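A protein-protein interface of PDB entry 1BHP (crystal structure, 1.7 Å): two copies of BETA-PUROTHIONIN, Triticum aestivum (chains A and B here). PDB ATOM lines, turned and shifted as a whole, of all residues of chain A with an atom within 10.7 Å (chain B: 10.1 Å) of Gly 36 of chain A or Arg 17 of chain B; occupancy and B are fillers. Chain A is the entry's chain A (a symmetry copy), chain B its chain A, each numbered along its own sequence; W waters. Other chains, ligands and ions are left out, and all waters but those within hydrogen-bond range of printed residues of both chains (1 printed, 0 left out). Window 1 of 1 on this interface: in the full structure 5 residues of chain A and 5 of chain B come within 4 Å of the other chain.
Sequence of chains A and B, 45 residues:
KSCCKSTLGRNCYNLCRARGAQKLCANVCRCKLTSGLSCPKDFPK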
ATOM      1  N   LYS A   1      33.002 -28.951 -21.258  1.00  0.00           N
ATOM      2  CA  LYS A   1      33.703 -29.033 -22.550  1.00  0.00           C
ATOM      3  C   LYS A   1      34.559 -27.773 -22.709  1.00  0.00           C
ATOM      4  O   LYS A   1      34.128 -26.693 -22.288  1.00  0.00           O
ATOM      5  CB  LYS A   1      32.753 -29.058 -23.733  1.00  0.00           C
ATOM      6  CG  LYS A   1      33.279 -29.835 -24.942  1.00  0.00           C
ATOM      7  CD  LYS A   1      32.309 -29.771 -26.095  1.00  0.00           C
ATOM      8  CE  LYS A   1      32.851 -30.329 -27.379  1.00  0.00           C
ATOM      9  NZ  LYS A   1      33.547 -31.628 -27.131  1.00  0.00           N
ATOM     10  N   SER A   2      35.734 -27.983 -23.317  1.00  0.00           N
ATOM     11  CA  SER A   2      36.570 -26.776 -23.538  1.00  0.00           C
ATOM     12  C   SER A   2      36.374 -26.491 -25.046  1.00  0.00           C
ATOM     13  O   SER A   2      36.295 -27.444 -25.816  1.00  0.00           O
ATOM     14  CB  SER A   2      38.030 -27.011 -23.253  1.00  0.00           C
ATOM     15  OG  SER A   2      38.425 -28.244 -23.854  1.00  0.00           O
ATOM     16  N   CYS A   3      36.361 -25.235 -25.348  1.00  0.00           N
ATOM     17  CA  CYS A   3      36.198 -24.748 -26.726  1.00  0.00           C
ATOM     18  C   CYS A   3      37.197 -23.633 -26.969  1.00  0.00           C
ATOM     19  O   CYS A   3      37.140 -22.583 -26.301  1.00  0.00           O
ATOM     20  CB  CYS A   3      34.764 -24.157 -26.858  1.00  0.00           C
ATOM     21  SG  CYS A   3      33.594 -25.486 -26.480  1.00  0.00           S
ATOM     22  N   LYS A  32      37.316 -21.338 -23.772  1.00  0.00           N
ATOM     23  CA  LYS A  32      36.099 -21.143 -22.931  1.00  0.00           C
ATOM     24  C   LYS A  32      35.642 -22.521 -22.484  1.00  0.00           C
ATOM     25  O   LYS A  32      35.799 -23.436 -23.299  1.00  0.00           O
ATOM     26  CB  LYS A  32      34.938 -20.551 -23.735  1.00  0.00           C
ATOM     27  CG  LYS A  32      34.744 -19.056 -23.621  1.00  0.00           C
ATOM     28  CD  LYS A  32      33.407 -18.573 -24.178  1.00  0.00           C
ATOM     29  CE  LYS A  32      33.107 -17.164 -23.595  1.00  0.00           C
ATOM     30  NZ  LYS A  32      34.398 -16.388 -23.610  1.00  0.00           N
ATOM     31  N   LEU A  33      35.137 -22.587 -21.278  1.00  0.00           N
ATOM     32  CA  LEU A  33      34.607 -23.911 -20.798  1.00  0.00           C
ATOM     33  C   LEU A  33      33.078 -23.755 -20.957  1.00  0.00           C
ATOM     34  O   LEU A  33      32.570 -22.663 -20.624  1.00  0.00           O
ATOM     35  CB  LEU A  33      35.091 -24.080 -19.374  1.00  0.00           C
ATOM     36  CG  LEU A  33      36.586 -24.335 -19.165  1.00  0.00           C
ATOM     37  CD1 LEU A  33      36.876 -24.459 -17.673  1.00  0.00           C
ATOM     38  CD2 LEU A  33      36.955 -25.602 -19.891  1.00  0.00           C
ATOM     39  N   THR A  34      32.417 -24.764 -21.462  1.00  0.00           N
ATOM     40  CA  THR A  34      30.945 -24.654 -21.605  1.00  0.00           C
ATOM     41  C   THR A  34      30.254 -25.821 -20.913  1.00  0.00           C
ATOM     42  O   THR A  34      30.905 -26.881 -20.823  1.00  0.00           O
ATOM     43  CB  THR A  34      30.516 -24.712 -23.137  1.00  0.00           C
ATOM     44  OG1 THR A  34      29.056 -24.596 -22.989  1.00  0.00           O
ATOM     45  CG2 THR A  34      30.871 -26.021 -23.834  1.00  0.00           C
ATOM     46  N   SER A  35      29.018 -25.642 -20.477  1.00  0.00           N
ATOM     47  CA  SER A  35      28.257 -26.726 -19.855  1.00  0.00           C
ATOM     48  C   SER A  35      27.539 -27.543 -20.937  1.00  0.00           C
ATOM     49  O   SER A  35      27.087 -28.689 -20.714  1.00  0.00           O
ATOM     50  CB  SER A  35      27.215 -26.219 -18.857  1.00  0.00           C
ATOM     51  OG  SER A  35      27.871 -25.809 -17.665  1.00  0.00           O
ATOM     52  N   GLY A  36      27.446 -26.947 -22.105  1.00  0.00           N
ATOM     53  CA  GLY A  36      26.792 -27.587 -23.269  1.00  0.00           C
ATOM     54  C   GLY A  36      27.648 -28.703 -23.798  1.00  0.00           C
ATOM     55  O   GLY A  36      28.851 -28.768 -23.539  1.00  0.00           O
ATOM     56  N   LEU A  37      27.081 -29.591 -24.575  1.00  0.00           N
ATOM     57  CA  LEU A  37      27.729 -30.719 -25.208  1.00  0.00           C
ATOM     58  C   LEU A  37      28.394 -30.356 -26.543  1.00  0.00           C
ATOM     59  O   LEU A  37      29.028 -31.254 -27.105  1.00  0.00           O
ATOM     60  CB  LEU A  37      26.681 -31.845 -25.396  1.00  0.00           C
ATOM     61  CG  LEU A  37      26.163 -32.507 -24.110  1.00  0.00           C
ATOM     62  CD1 LEU A  37      24.662 -32.736 -24.202  1.00  0.00           C
ATOM     63  CD2 LEU A  37      26.807 -33.901 -24.025  1.00  0.00           C
ATOM     64  N   SER A  38      28.207 -29.134 -26.991  1.00  0.00           N
ATOM     65  CA  SER A  38      28.825 -28.656 -28.258  1.00  0.00           C
ATOM     66  C   SER A  38      29.426 -27.275 -28.036  1.00  0.00           C
ATOM     67  O   SER A  38      29.093 -26.575 -27.082  1.00  0.00           O
ATOM     68  CB  SER A  38      27.859 -28.694 -29.425  1.00  0.00           C
ATOM     69  OG  SER A  38      27.833 -30.018 -29.936  1.00  0.00           O
ATOM     70  N   CYS A  39      30.340 -26.901 -28.927  1.00  0.00           N
ATOM     71  CA  CYS A  39      31.027 -25.597 -28.811  1.00  0.00           C
ATOM     72  C   CYS A  39      30.311 -24.584 -29.705  1.00  0.00           C
ATOM     73  O   CYS A  39      29.784 -25.037 -30.700  1.00  0.00           O
ATOM     74  CB  CYS A  39      32.485 -25.787 -29.229  1.00  0.00           C
ATOM     75  SG  CYS A  39      33.513 -26.679 -28.004  1.00  0.00           S
ATOM     76  N   PRO A  40      30.337 -23.349 -29.266  1.00  0.00           N
ATOM     77  CA  PRO A  40      29.723 -22.243 -30.036  1.00  0.00           C
ATOM     78  C   PRO A  40      30.559 -22.102 -31.308  1.00  0.00           C
ATOM     79  O   PRO A  40      31.685 -22.607 -31.371  1.00  0.00           O
ATOM     80  CB  PRO A  40      29.785 -21.055 -29.124  1.00  0.00           C
ATOM     81  CG  PRO A  40      30.449 -21.460 -27.855  1.00  0.00           C
ATOM     82  CD  PRO A  40      30.992 -22.861 -28.048  1.00  0.00           C
ATOM     83  N   PHE A  43      34.143 -20.555 -31.105  1.00  0.00           N
ATOM     84  CA  PHE A  43      35.175 -21.266 -30.298  1.00  0.00           C
ATOM     85  C   PHE A  43      35.115 -22.720 -30.772  1.00  0.00           C
ATOM     86  O   PHE A  43      34.780 -23.585 -29.966  1.00  0.00           O
ATOM     87  CB  PHE A  43      34.865 -21.192 -28.814  1.00  0.00           C
ATOM     88  CG  PHE A  43      35.241 -19.896 -28.171  1.00  0.00           C
ATOM     89  CD1 PHE A  43      34.344 -18.828 -28.164  1.00  0.00           C
ATOM     90  CD2 PHE A  43      36.506 -19.734 -27.597  1.00  0.00           C
ATOM     91  CE1 PHE A  43      34.694 -17.620 -27.595  1.00  0.00           C
ATOM     92  CE2 PHE A  43      36.881 -18.537 -27.011  1.00  0.00           C
ATOM     93  CZ  PHE A  43      35.947 -17.477 -27.026  1.00  0.00           C
ATOM     94  N   LYS B   1      19.405 -37.420 -13.528  1.00  0.00           N
ATOM     95  CA  LYS B   1      18.580 -37.889 -14.653  1.00  0.00           C
ATOM     96  C   LYS B   1      17.576 -36.787 -15.002  1.00  0.00           C
ATOM     97  O   LYS B   1      17.083 -36.109 -14.092  1.00  0.00           O
ATOM     98  CB  LYS B   1      17.762 -39.120 -14.307  1.00  0.00           C
ATOM     99  CG  LYS B   1      17.492 -40.047 -15.495  1.00  0.00           C
ATOM    100  CD  LYS B   1      16.630 -41.216 -15.090  1.00  0.00           C
ATOM    101  CE  LYS B   1      16.151 -42.049 -16.242  1.00  0.00           C
ATOM    102  NZ  LYS B   1      17.270 -42.312 -17.197  1.00  0.00           N
ATOM    103  N   SER B   2      17.326 -36.670 -16.313  1.00  0.00           N
ATOM    104  CA  SER B   2      16.317 -35.648 -16.687  1.00  0.00           C
ATOM    105  C   SER B   2      15.063 -36.497 -17.000  1.00  0.00           C
ATOM    106  O   SER B   2      15.213 -37.577 -17.565  1.00  0.00           O
ATOM    107  CB  SER B   2      16.708 -34.853 -17.906  1.00  0.00           C
ATOM    108  OG  SER B   2      17.186 -35.751 -18.907  1.00  0.00           O
ATOM    109  N   CYS B   4      11.213 -35.778 -18.637  1.00  0.00           N
ATOM    110  CA  CYS B   4      10.308 -34.848 -19.310  1.00  0.00           C
ATOM    111  C   CYS B   4       8.861 -35.322 -19.299  1.00  0.00           C
ATOM    112  O   CYS B   4       8.557 -36.520 -19.207  1.00  0.00           O
ATOM    113  CB  CYS B   4      10.860 -34.618 -20.725  1.00  0.00           C
ATOM    114  SG  CYS B   4      12.556 -33.873 -20.725  1.00  0.00           S
ATOM    115  N   GLY B   9       8.989 -31.998 -25.129  1.00  0.00           N
ATOM    116  CA  GLY B   9       9.862 -31.496 -24.053  1.00  0.00           C
ATOM    117  C   GLY B   9      11.171 -32.309 -24.117  1.00  0.00           C
ATOM    118  O   GLY B   9      12.223 -31.711 -23.889  1.00  0.00           O
ATOM    119  N   ARG B  10      11.098 -33.577 -24.439  1.00  0.00           N
ATOM    120  CA  ARG B  10      12.340 -34.382 -24.545  1.00  0.00           C
ATOM    121  C   ARG B  10      13.203 -33.845 -25.691  1.00  0.00           C
ATOM    122  O   ARG B  10      14.419 -33.570 -25.511  1.00  0.00           O
ATOM    123  CB  ARG B  10      12.066 -35.894 -24.687  1.00  0.00           C
ATOM    124  CG  ARG B  10      13.365 -36.673 -25.055  1.00  0.00           C
ATOM    125  CD  ARG B  10      14.406 -36.557 -23.980  1.00  0.00           C
ATOM    126  NE  ARG B  10      14.026 -36.988 -22.661  1.00  0.00           N
ATOM    127  CZ  ARG B  10      14.805 -36.781 -21.585  1.00  0.00           C
ATOM    128  NH1 ARG B  10      16.016 -36.245 -21.679  1.00  0.00           N
ATOM    129  NH2 ARG B  10      14.351 -37.142 -20.386  1.00  0.00           N
ATOM    130  N   ASN B  11      12.610 -33.642 -26.871  1.00  0.00           N
ATOM    131  CA  ASN B  11      13.420 -33.104 -28.027  1.00  0.00           C
ATOM    132  C   ASN B  11      13.930 -31.740 -27.627  1.00  0.00           C
ATOM    133  O   ASN B  11      15.081 -31.336 -27.945  1.00  0.00           O
ATOM    134  CB  ASN B  11      12.536 -33.149 -29.276  1.00  0.00           C
ATOM    135  CG  ASN B  11      12.538 -34.488 -29.931  1.00  0.00           C
ATOM    136  OD1 ASN B  11      12.441 -35.585 -29.296  1.00  0.00           O
ATOM    137  ND2 ASN B  11      12.685 -34.542 -31.237  1.00  0.00           N
ATOM    138  N   CYS B  12      13.075 -31.006 -26.944  1.00  0.00           N
ATOM    139  CA  CYS B  12      13.455 -29.655 -26.498  1.00  0.00           C
ATOM    140  C   CYS B  12      14.717 -29.738 -25.617  1.00  0.00           C
ATOM    141  O   CYS B  12      15.649 -28.948 -25.857  1.00  0.00           O
ATOM    142  CB  CYS B  12      12.361 -28.933 -25.765  1.00  0.00           C
ATOM    143  SG  CYS B  12      12.709 -27.300 -25.101  1.00  0.00           S
ATOM    144  N   TYR B  13      14.673 -30.603 -24.623  1.00  0.00           N
ATOM    145  CA  TYR B  13      15.820 -30.700 -23.690  1.00  0.00           C
ATOM    146  C   TYR B  13      17.069 -31.126 -24.382  1.00  0.00           C
ATOM    147  O   TYR B  13      18.151 -30.505 -24.214  1.00  0.00           O
ATOM    148  CB  TYR B  13      15.421 -31.666 -22.539  1.00  0.00           C
ATOM    149  CG  TYR B  13      16.504 -31.863 -21.528  1.00  0.00           C
ATOM    150  CD1 TYR B  13      17.455 -32.858 -21.629  1.00  0.00           C
ATOM    151  CD2 TYR B  13      16.526 -30.987 -20.434  1.00  0.00           C
ATOM    152  CE1 TYR B  13      18.477 -33.028 -20.661  1.00  0.00           C
ATOM    153  CE2 TYR B  13      17.520 -31.148 -19.445  1.00  0.00           C
ATOM    154  CZ  TYR B  13      18.456 -32.138 -19.581  1.00  0.00           C
ATOM    155  OH  TYR B  13      19.408 -32.214 -18.583  1.00  0.00           O
ATOM    156  N   ASN B  14      17.005 -32.188 -25.186  1.00  0.00           N
ATOM    157  CA  ASN B  14      18.190 -32.695 -25.866  1.00  0.00           C
ATOM    158  C   ASN B  14      18.845 -31.641 -26.755  1.00  0.00           C
ATOM    159  O   ASN B  14      20.081 -31.608 -26.842  1.00  0.00           O
ATOM    160  CB  ASN B  14      17.907 -33.985 -26.632  1.00  0.00           C
ATOM    161  CG  ASN B  14      17.611 -35.173 -25.818  1.00  0.00           C
ATOM    162  OD1 ASN B  14      17.663 -35.058 -24.568  1.00  0.00           O
ATOM    163  ND2 ASN B  14      17.276 -36.321 -26.434  1.00  0.00           N
ATOM    164  N   LEU B  15      18.041 -30.846 -27.434  1.00  0.00           N
ATOM    165  CA  LEU B  15      18.605 -29.794 -28.361  1.00  0.00           C
ATOM    166  C   LEU B  15      19.201 -28.691 -27.533  1.00  0.00           C
ATOM    167  O   LEU B  15      20.319 -28.158 -27.844  1.00  0.00           O
ATOM    168  CB  LEU B  15      17.398 -29.289 -29.167  1.00  0.00           C
ATOM    169  CG  LEU B  15      16.991 -29.859 -30.479  1.00  0.00           C
ATOM    170  CD1 LEU B  15      16.230 -28.957 -31.403  1.00  0.00           C
ATOM    171  CD2 LEU B  15      18.250 -30.280 -31.247  1.00  0.00           C
ATOM    172  N   CYS B  16      18.478 -28.355 -26.489  1.00  0.00           N
ATOM    173  CA  CYS B  16      18.933 -27.280 -25.563  1.00  0.00           C
ATOM    174  C   CYS B  16      20.290 -27.608 -24.967  1.00  0.00           C
ATOM    175  O   CYS B  16      21.119 -26.707 -24.795  1.00  0.00           O
ATOM    176  CB  CYS B  16      17.871 -26.959 -24.513  1.00  0.00           C
ATOM    177  SG  CYS B  16      18.341 -25.746 -23.250  1.00  0.00           S
ATOM    178  N   ARG B  17      20.547 -28.859 -24.624  1.00  0.00           N
ATOM    179  CA  ARG B  17      21.789 -29.282 -24.005  1.00  0.00           C
ATOM    180  C   ARG B  17      22.986 -29.102 -24.897  1.00  0.00           C
ATOM    181  O   ARG B  17      24.095 -29.305 -24.420  1.00  0.00           O
ATOM    182  CB  ARG B  17      21.714 -30.712 -23.478  1.00  0.00           C
ATOM    183  CG  ARG B  17      20.790 -30.826 -22.234  1.00  0.00           C
ATOM    184  CD  ARG B  17      21.531 -30.304 -21.008  1.00  0.00           C
ATOM    185  NE  ARG B  17      22.569 -31.298 -20.723  1.00  0.00           N
ATOM    186  CZ  ARG B  17      23.870 -31.003 -20.582  1.00  0.00           C
ATOM    187  NH1 ARG B  17      24.350 -29.782 -20.716  1.00  0.00           N
ATOM    188  NH2 ARG B  17      24.678 -32.037 -20.332  1.00  0.00           N
ATOM    189  N   ALA B  18      22.747 -28.771 -26.179  1.00  0.00           N
ATOM    190  CA  ALA B  18      23.902 -28.561 -27.083  1.00  0.00           C
ATOM    191  C   ALA B  18      24.638 -27.328 -26.598  1.00  0.00           C
ATOM    192  O   ALA B  18      25.892 -27.258 -26.699  1.00  0.00           O
ATOM    193  CB  ALA B  18      23.446 -28.325 -28.539  1.00  0.00           C
ATOM    194  N   ARG B  19      23.952 -26.369 -26.047  1.00  0.00           N
ATOM    195  CA  ARG B  19      24.544 -25.133 -25.566  1.00  0.00           C
ATOM    196  C   ARG B  19      24.220 -24.704 -24.174  1.00  0.00           C
ATOM    197  O   ARG B  19      24.813 -23.739 -23.700  1.00  0.00           O
ATOM    198  CB  ARG B  19      24.110 -23.986 -26.549  1.00  0.00           C
ATOM    199  CG  ARG B  19      24.410 -24.325 -28.015  1.00  0.00           C
ATOM    200  CD  ARG B  19      25.749 -23.734 -28.402  1.00  0.00           C
ATOM    201  NE  ARG B  19      26.423 -24.522 -29.409  1.00  0.00           N
ATOM    202  CZ  ARG B  19      26.184 -24.575 -30.705  1.00  0.00           C
ATOM    203  NH1 ARG B  19      25.130 -23.936 -31.239  1.00  0.00           N
ATOM    204  NH2 ARG B  19      26.978 -25.218 -31.563  1.00  0.00           N
ATOM    205  N   GLY B  20      23.301 -25.367 -23.480  1.00  0.00           N
ATOM    206  CA  GLY B  20      22.896 -24.989 -22.151  1.00  0.00           C
ATOM    207  C   GLY B  20      23.149 -26.059 -21.113  1.00  0.00           C
ATOM    208  O   GLY B  20      23.442 -27.213 -21.422  1.00  0.00           O
ATOM    209  N   ALA B  21      23.076 -25.605 -19.876  1.00  0.00           N
ATOM    210  CA  ALA B  21      23.277 -26.496 -18.712  1.00  0.00           C
ATOM    211  C   ALA B  21      22.014 -27.330 -18.481  1.00  0.00           C
ATOM    212  O   ALA B  21      20.928 -26.914 -18.934  1.00  0.00           O
ATOM    213  CB  ALA B  21      23.542 -25.608 -17.496  1.00  0.00           C
ATOM    214  N   GLN B  22      22.174 -28.418 -17.760  1.00  0.00           N
ATOM    215  CA  GLN B  22      21.029 -29.304 -17.415  1.00  0.00           C
ATOM    216  C   GLN B  22      19.882 -28.499 -16.805  1.00  0.00           C
ATOM    217  O   GLN B  22      18.766 -28.496 -17.297  1.00  0.00           O
ATOM    218  CB  GLN B  22      21.430 -30.416 -16.451  1.00  0.00           C
ATOM    219  CG  GLN B  22      22.655 -31.220 -16.891  1.00  0.00           C
ATOM    220  CD  GLN B  22      22.895 -32.407 -15.975  1.00  0.00           C
ATOM    221  OE1 GLN B  22      23.204 -33.516 -16.415  1.00  0.00           O
ATOM    222  NE2 GLN B  22      22.737 -32.147 -14.673  1.00  0.00           N
ATOM    223  N   LYS B  23      20.135 -27.818 -15.730  1.00  0.00           N
ATOM    224  CA  LYS B  23      19.228 -27.007 -14.934  1.00  0.00           C
ATOM    225  C   LYS B  23      18.521 -25.947 -15.711  1.00  0.00           C
ATOM    226  O   LYS B  23      17.308 -25.771 -15.453  1.00  0.00           O
ATOM    227  CB  LYS B  23      19.821 -26.457 -13.646  1.00  0.00           C
ATOM    228  CG  LYS B  23      19.920 -27.429 -12.470  1.00  0.00           C
ATOM    229  CD  LYS B  23      19.876 -26.678 -11.146  1.00  0.00           C
ATOM    230  CE  LYS B  23      20.563 -27.354  -9.981  1.00  0.00           C
ATOM    231  NZ  LYS B  23      19.676 -28.338  -9.297  1.00  0.00           N
ATOM    232  N   LEU B  24      19.180 -25.250 -16.634  1.00  0.00           N
ATOM    233  CA  LEU B  24      18.460 -24.221 -17.422  1.00  0.00           C
ATOM    234  C   LEU B  24      17.576 -24.874 -18.476  1.00  0.00           C
ATOM    235  O   LEU B  24      16.467 -24.420 -18.774  1.00  0.00           O
ATOM    236  CB  LEU B  24      19.556 -23.332 -18.068  1.00  0.00           C
ATOM    237  CG  LEU B  24      19.023 -22.473 -19.196  1.00  0.00           C
ATOM    238  CD1 LEU B  24      18.339 -21.239 -18.612  1.00  0.00           C
ATOM    239  CD2 LEU B  24      20.194 -22.081 -20.110  1.00  0.00           C
ATOM    240  N   CYS B  25      18.086 -25.935 -19.079  1.00  0.00           N
ATOM    241  CA  CYS B  25      17.350 -26.687 -20.111  1.00  0.00           C
ATOM    242  C   CYS B  25      16.112 -27.365 -19.545  1.00  0.00           C
ATOM    243  O   CYS B  25      15.089 -27.426 -20.223  1.00  0.00           O
ATOM    244  CB  CYS B  25      18.294 -27.644 -20.848  1.00  0.00           C
ATOM    245  SG  CYS B  25      19.447 -26.790 -21.928  1.00  0.00           S
ATOM    246  N   ALA B  26      16.222 -27.878 -18.330  1.00  0.00           N
ATOM    247  CA  ALA B  26      15.081 -28.548 -17.659  1.00  0.00           C
ATOM    248  C   ALA B  26      13.952 -27.531 -17.533  1.00  0.00           C
ATOM    249  O   ALA B  26      12.823 -27.844 -17.908  1.00  0.00           O
ATOM    250  CB  ALA B  26      15.491 -29.107 -16.324  1.00  0.00           C
ATOM    251  N   ASN B  27      14.267 -26.346 -17.052  1.00  0.00           N
ATOM    252  CA  ASN B  27      13.330 -25.254 -16.871  1.00  0.00           C
ATOM    253  C   ASN B  27      12.579 -24.810 -18.115  1.00  0.00           C
ATOM    254  O   ASN B  27      11.329 -24.709 -18.084  1.00  0.00           O
ATOM    255  CB  ASN B  27      14.022 -24.001 -16.249  1.00  0.00           C
ATOM    256  CG  ASN B  27      14.189 -24.173 -14.755  1.00  0.00           C
ATOM    257  OD1 ASN B  27      15.304 -24.358 -14.256  1.00  0.00           O
ATOM    258  ND2 ASN B  27      13.080 -24.115 -14.018  1.00  0.00           N
ATOM    259  N   VAL B  28      13.323 -24.541 -19.164  1.00  0.00           N
ATOM    260  CA  VAL B  28      12.776 -24.061 -20.419  1.00  0.00           C
ATOM    261  C   VAL B  28      12.009 -25.141 -21.169  1.00  0.00           C
ATOM    262  O   VAL B  28      11.100 -24.789 -21.954  1.00  0.00           O
ATOM    263  CB  VAL B  28      13.903 -23.447 -21.282  1.00  0.00           C
ATOM    264  CG1 VAL B  28      13.448 -23.157 -22.690  1.00  0.00           C
ATOM    265  CG2 VAL B  28      14.561 -22.239 -20.624  1.00  0.00           C
ATOM    266  N   CYS B  29      12.396 -26.399 -20.983  1.00  0.00           N
ATOM    267  CA  CYS B  29      11.693 -27.485 -21.717  1.00  0.00           C
ATOM    268  C   CYS B  29      10.690 -28.200 -20.818  1.00  0.00           C
ATOM    269  O   CYS B  29      10.139 -29.252 -21.210  1.00  0.00           O
ATOM    270  CB  CYS B  29      12.726 -28.416 -22.329  1.00  0.00           C
ATOM    271  SG  CYS B  29      13.880 -27.613 -23.497  1.00  0.00           S
ATOM    272  N   CYS B  31      11.041 -29.852 -17.978  1.00  0.00           N
ATOM    273  CA  CYS B  31      11.513 -31.166 -17.551  1.00  0.00           C
ATOM    274  C   CYS B  31      11.941 -31.025 -16.102  1.00  0.00           C
ATOM    275  O   CYS B  31      11.952 -29.902 -15.573  1.00  0.00           O
ATOM    276  CB  CYS B  31      12.635 -31.754 -18.419  1.00  0.00           C
ATOM    277  SG  CYS B  31      12.248 -31.988 -20.127  1.00  0.00           S
ATOM    278  N   LEU B  33      14.842 -32.513 -13.121  1.00  0.00           N
ATOM    279  CA  LEU B  33      16.120 -33.289 -12.949  1.00  0.00           C
ATOM    280  C   LEU B  33      15.872 -34.090 -11.652  1.00  0.00           C
ATOM    281  O   LEU B  33      15.308 -33.498 -10.706  1.00  0.00           O
ATOM    282  CB  LEU B  33      17.237 -32.271 -12.873  1.00  0.00           C
ATOM    283  CG  LEU B  33      17.591 -31.517 -14.158  1.00  0.00           C
ATOM    284  CD1 LEU B  33      18.719 -30.531 -13.874  1.00  0.00           C
ATOM    285  CD2 LEU B  33      18.007 -32.524 -15.197  1.00  0.00           C
HETATM  286  O   HOH W   1      27.482 -31.109 -19.314  1.00  0.00           O
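NH1 of Arg 17 of chain B is in hydrogen-bond range of O of Ser 35 of chain A (2.9 Å). The backbone NH (N) of Leu 37 of chain A sits at hydrogen-bond distance from the backbone carbonyl oxygen (O) of Arg 17 of chain B, at 3.0 Å. The backbone NH (N) of Leu 37 of chain A sits at hydrogen-bond distance from the backbone carbonyl oxygen (O) of Ala 18 of chain B. The backbone NH (N) of Ser 38 of chain A lies within hydrogen-bond range of the backbone carbonyl oxygen (O) of Ala 18 of chain B, 3.0 Å away. The guanidinium group (NH2) of Arg 19 of chain B sits at hydrogen-bond distance from the backbone carbonyl oxygen (O) of Cys 39 of chain A, at 2.9 Å.
The guanidinium group of Arg 17 of chain B lies within hydrogen-bond range of the backbone carbonyl oxygen of Gly 20 of chain B. N of Arg 17 of chain B lies within hydrogen-bond range of SG of Cys 25 of chain B (3.6 Å). The side-chain sulfur (SG) of Cys 3 of chain A forms a disulfide with the side-chain sulfur (SG) of Cys 39 of chain A (1.9 Å). OG1 of Thr 34 of chain A is in hydrogen-bond range of N of Gly 36 of chain A (3.0 Å). The side-chain sulfur of Cys 12 of chain B is disulfide-bonded to the side-chain sulfur of Cys 29 of chain B (2.0 Å). The side-chain sulfur (SG) of Cys 16 of chain B forms a disulfide with the side-chain sulfur (SG) of Cys 25 of chain B, 2.0 Å away.
O of Ser 35 of chain A touches O of Gly 20 of chain B, at 3.996 Å. Ala 21 of chain B touches Ser 35 of chain A (CA to CB, 3.95 Å). O of Arg 17 of chain B touches CA of Gly 36 of chain A (3.4 Å). O of Ala 18 of chain B touches CA of Gly 36 of chain A, 3.6 Å away. C of Arg 19 of chain B touches CA of Gly 36 of chain A (3.97 Å). Gly 36 of chain A touches Gly 20 of chain B.
Printed residues of chain B within 4 Å of Ser 35 of chain A: Arg 17, Gly 20 and Ala 21. Gly 36 of chain A touches just these residues of chain B: Arg 17 (3.4 Å), Ala 18 (3.6 Å), Arg 19 (3.97 Å) and Gly 20 (3.8 Å). Of chain B, only Arg 17 (3.0 Å) and Ala 18 (3.4 Å) come within 4 Å of Leu 37 of chain A. Of the printed residues of chain B, Ser 38 of chain A touches Ala 18. Printed residues of chain B within 4 Å of Cys 39 of chain A: Arg 19. Lys 1 of chain B touches none of the printed residues of chain A. Cys 4 of chain B touches none of the printed residues of chain A. No residue of chain A comes within 4 Å of Tyr 13 of chain B. Printed residues of chain A within 4 Å of Arg 17 of chain B: Ser 35 (2.9 Å), Gly 36 (3.4 Å) and Leu 37 (3.0 Å). Printed residues of chain A within 4 Å of Ala 18 of chain B: Gly 36 (3.6 Å), Leu 37 (3.4 Å) and Ser 38 (3.0 Å). Of the printed residues of chain A, Arg 19 of chain B touches Gly 36 (3.97 Å) and Cys 39 (2.9 Å). Of the printed residues of chain A, Gly 20 of chain B touches Ser 35 and Gly 36. Ala 21 of chain B touches one residue of chain A. No residue of chain A comes within 4 Å of Gln 22 of chain B. The nearest residue of chain B that does not touch Gly 36 of chain A is Ala 21 of chain B (5.1 Å). The nearest residue of chain A that does not touch Arg 17 of chain B is Ser 38 of chain A (4.9 Å).
Of the 26 printed residues of chain B, 5 touch a printed residue of chain A. Printed residues of chain A that touch a printed residue of chain B: Ser 35, Gly 36, Leu 37, Ser 38 and Cys 39. Among the printed residues, no Asp or Glu carboxylate lies within 4 Å of a Lys or Arg side-chain nitrogen of the other chain.
3 positions are printed for both chains. Of the 11 pairs that touch across the chains among the printed residues, none has its exchanged pair printed and touching as well.
Water W1 bridges O of Ser 35 of chain A and NH2 of Arg 17 of chain B.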
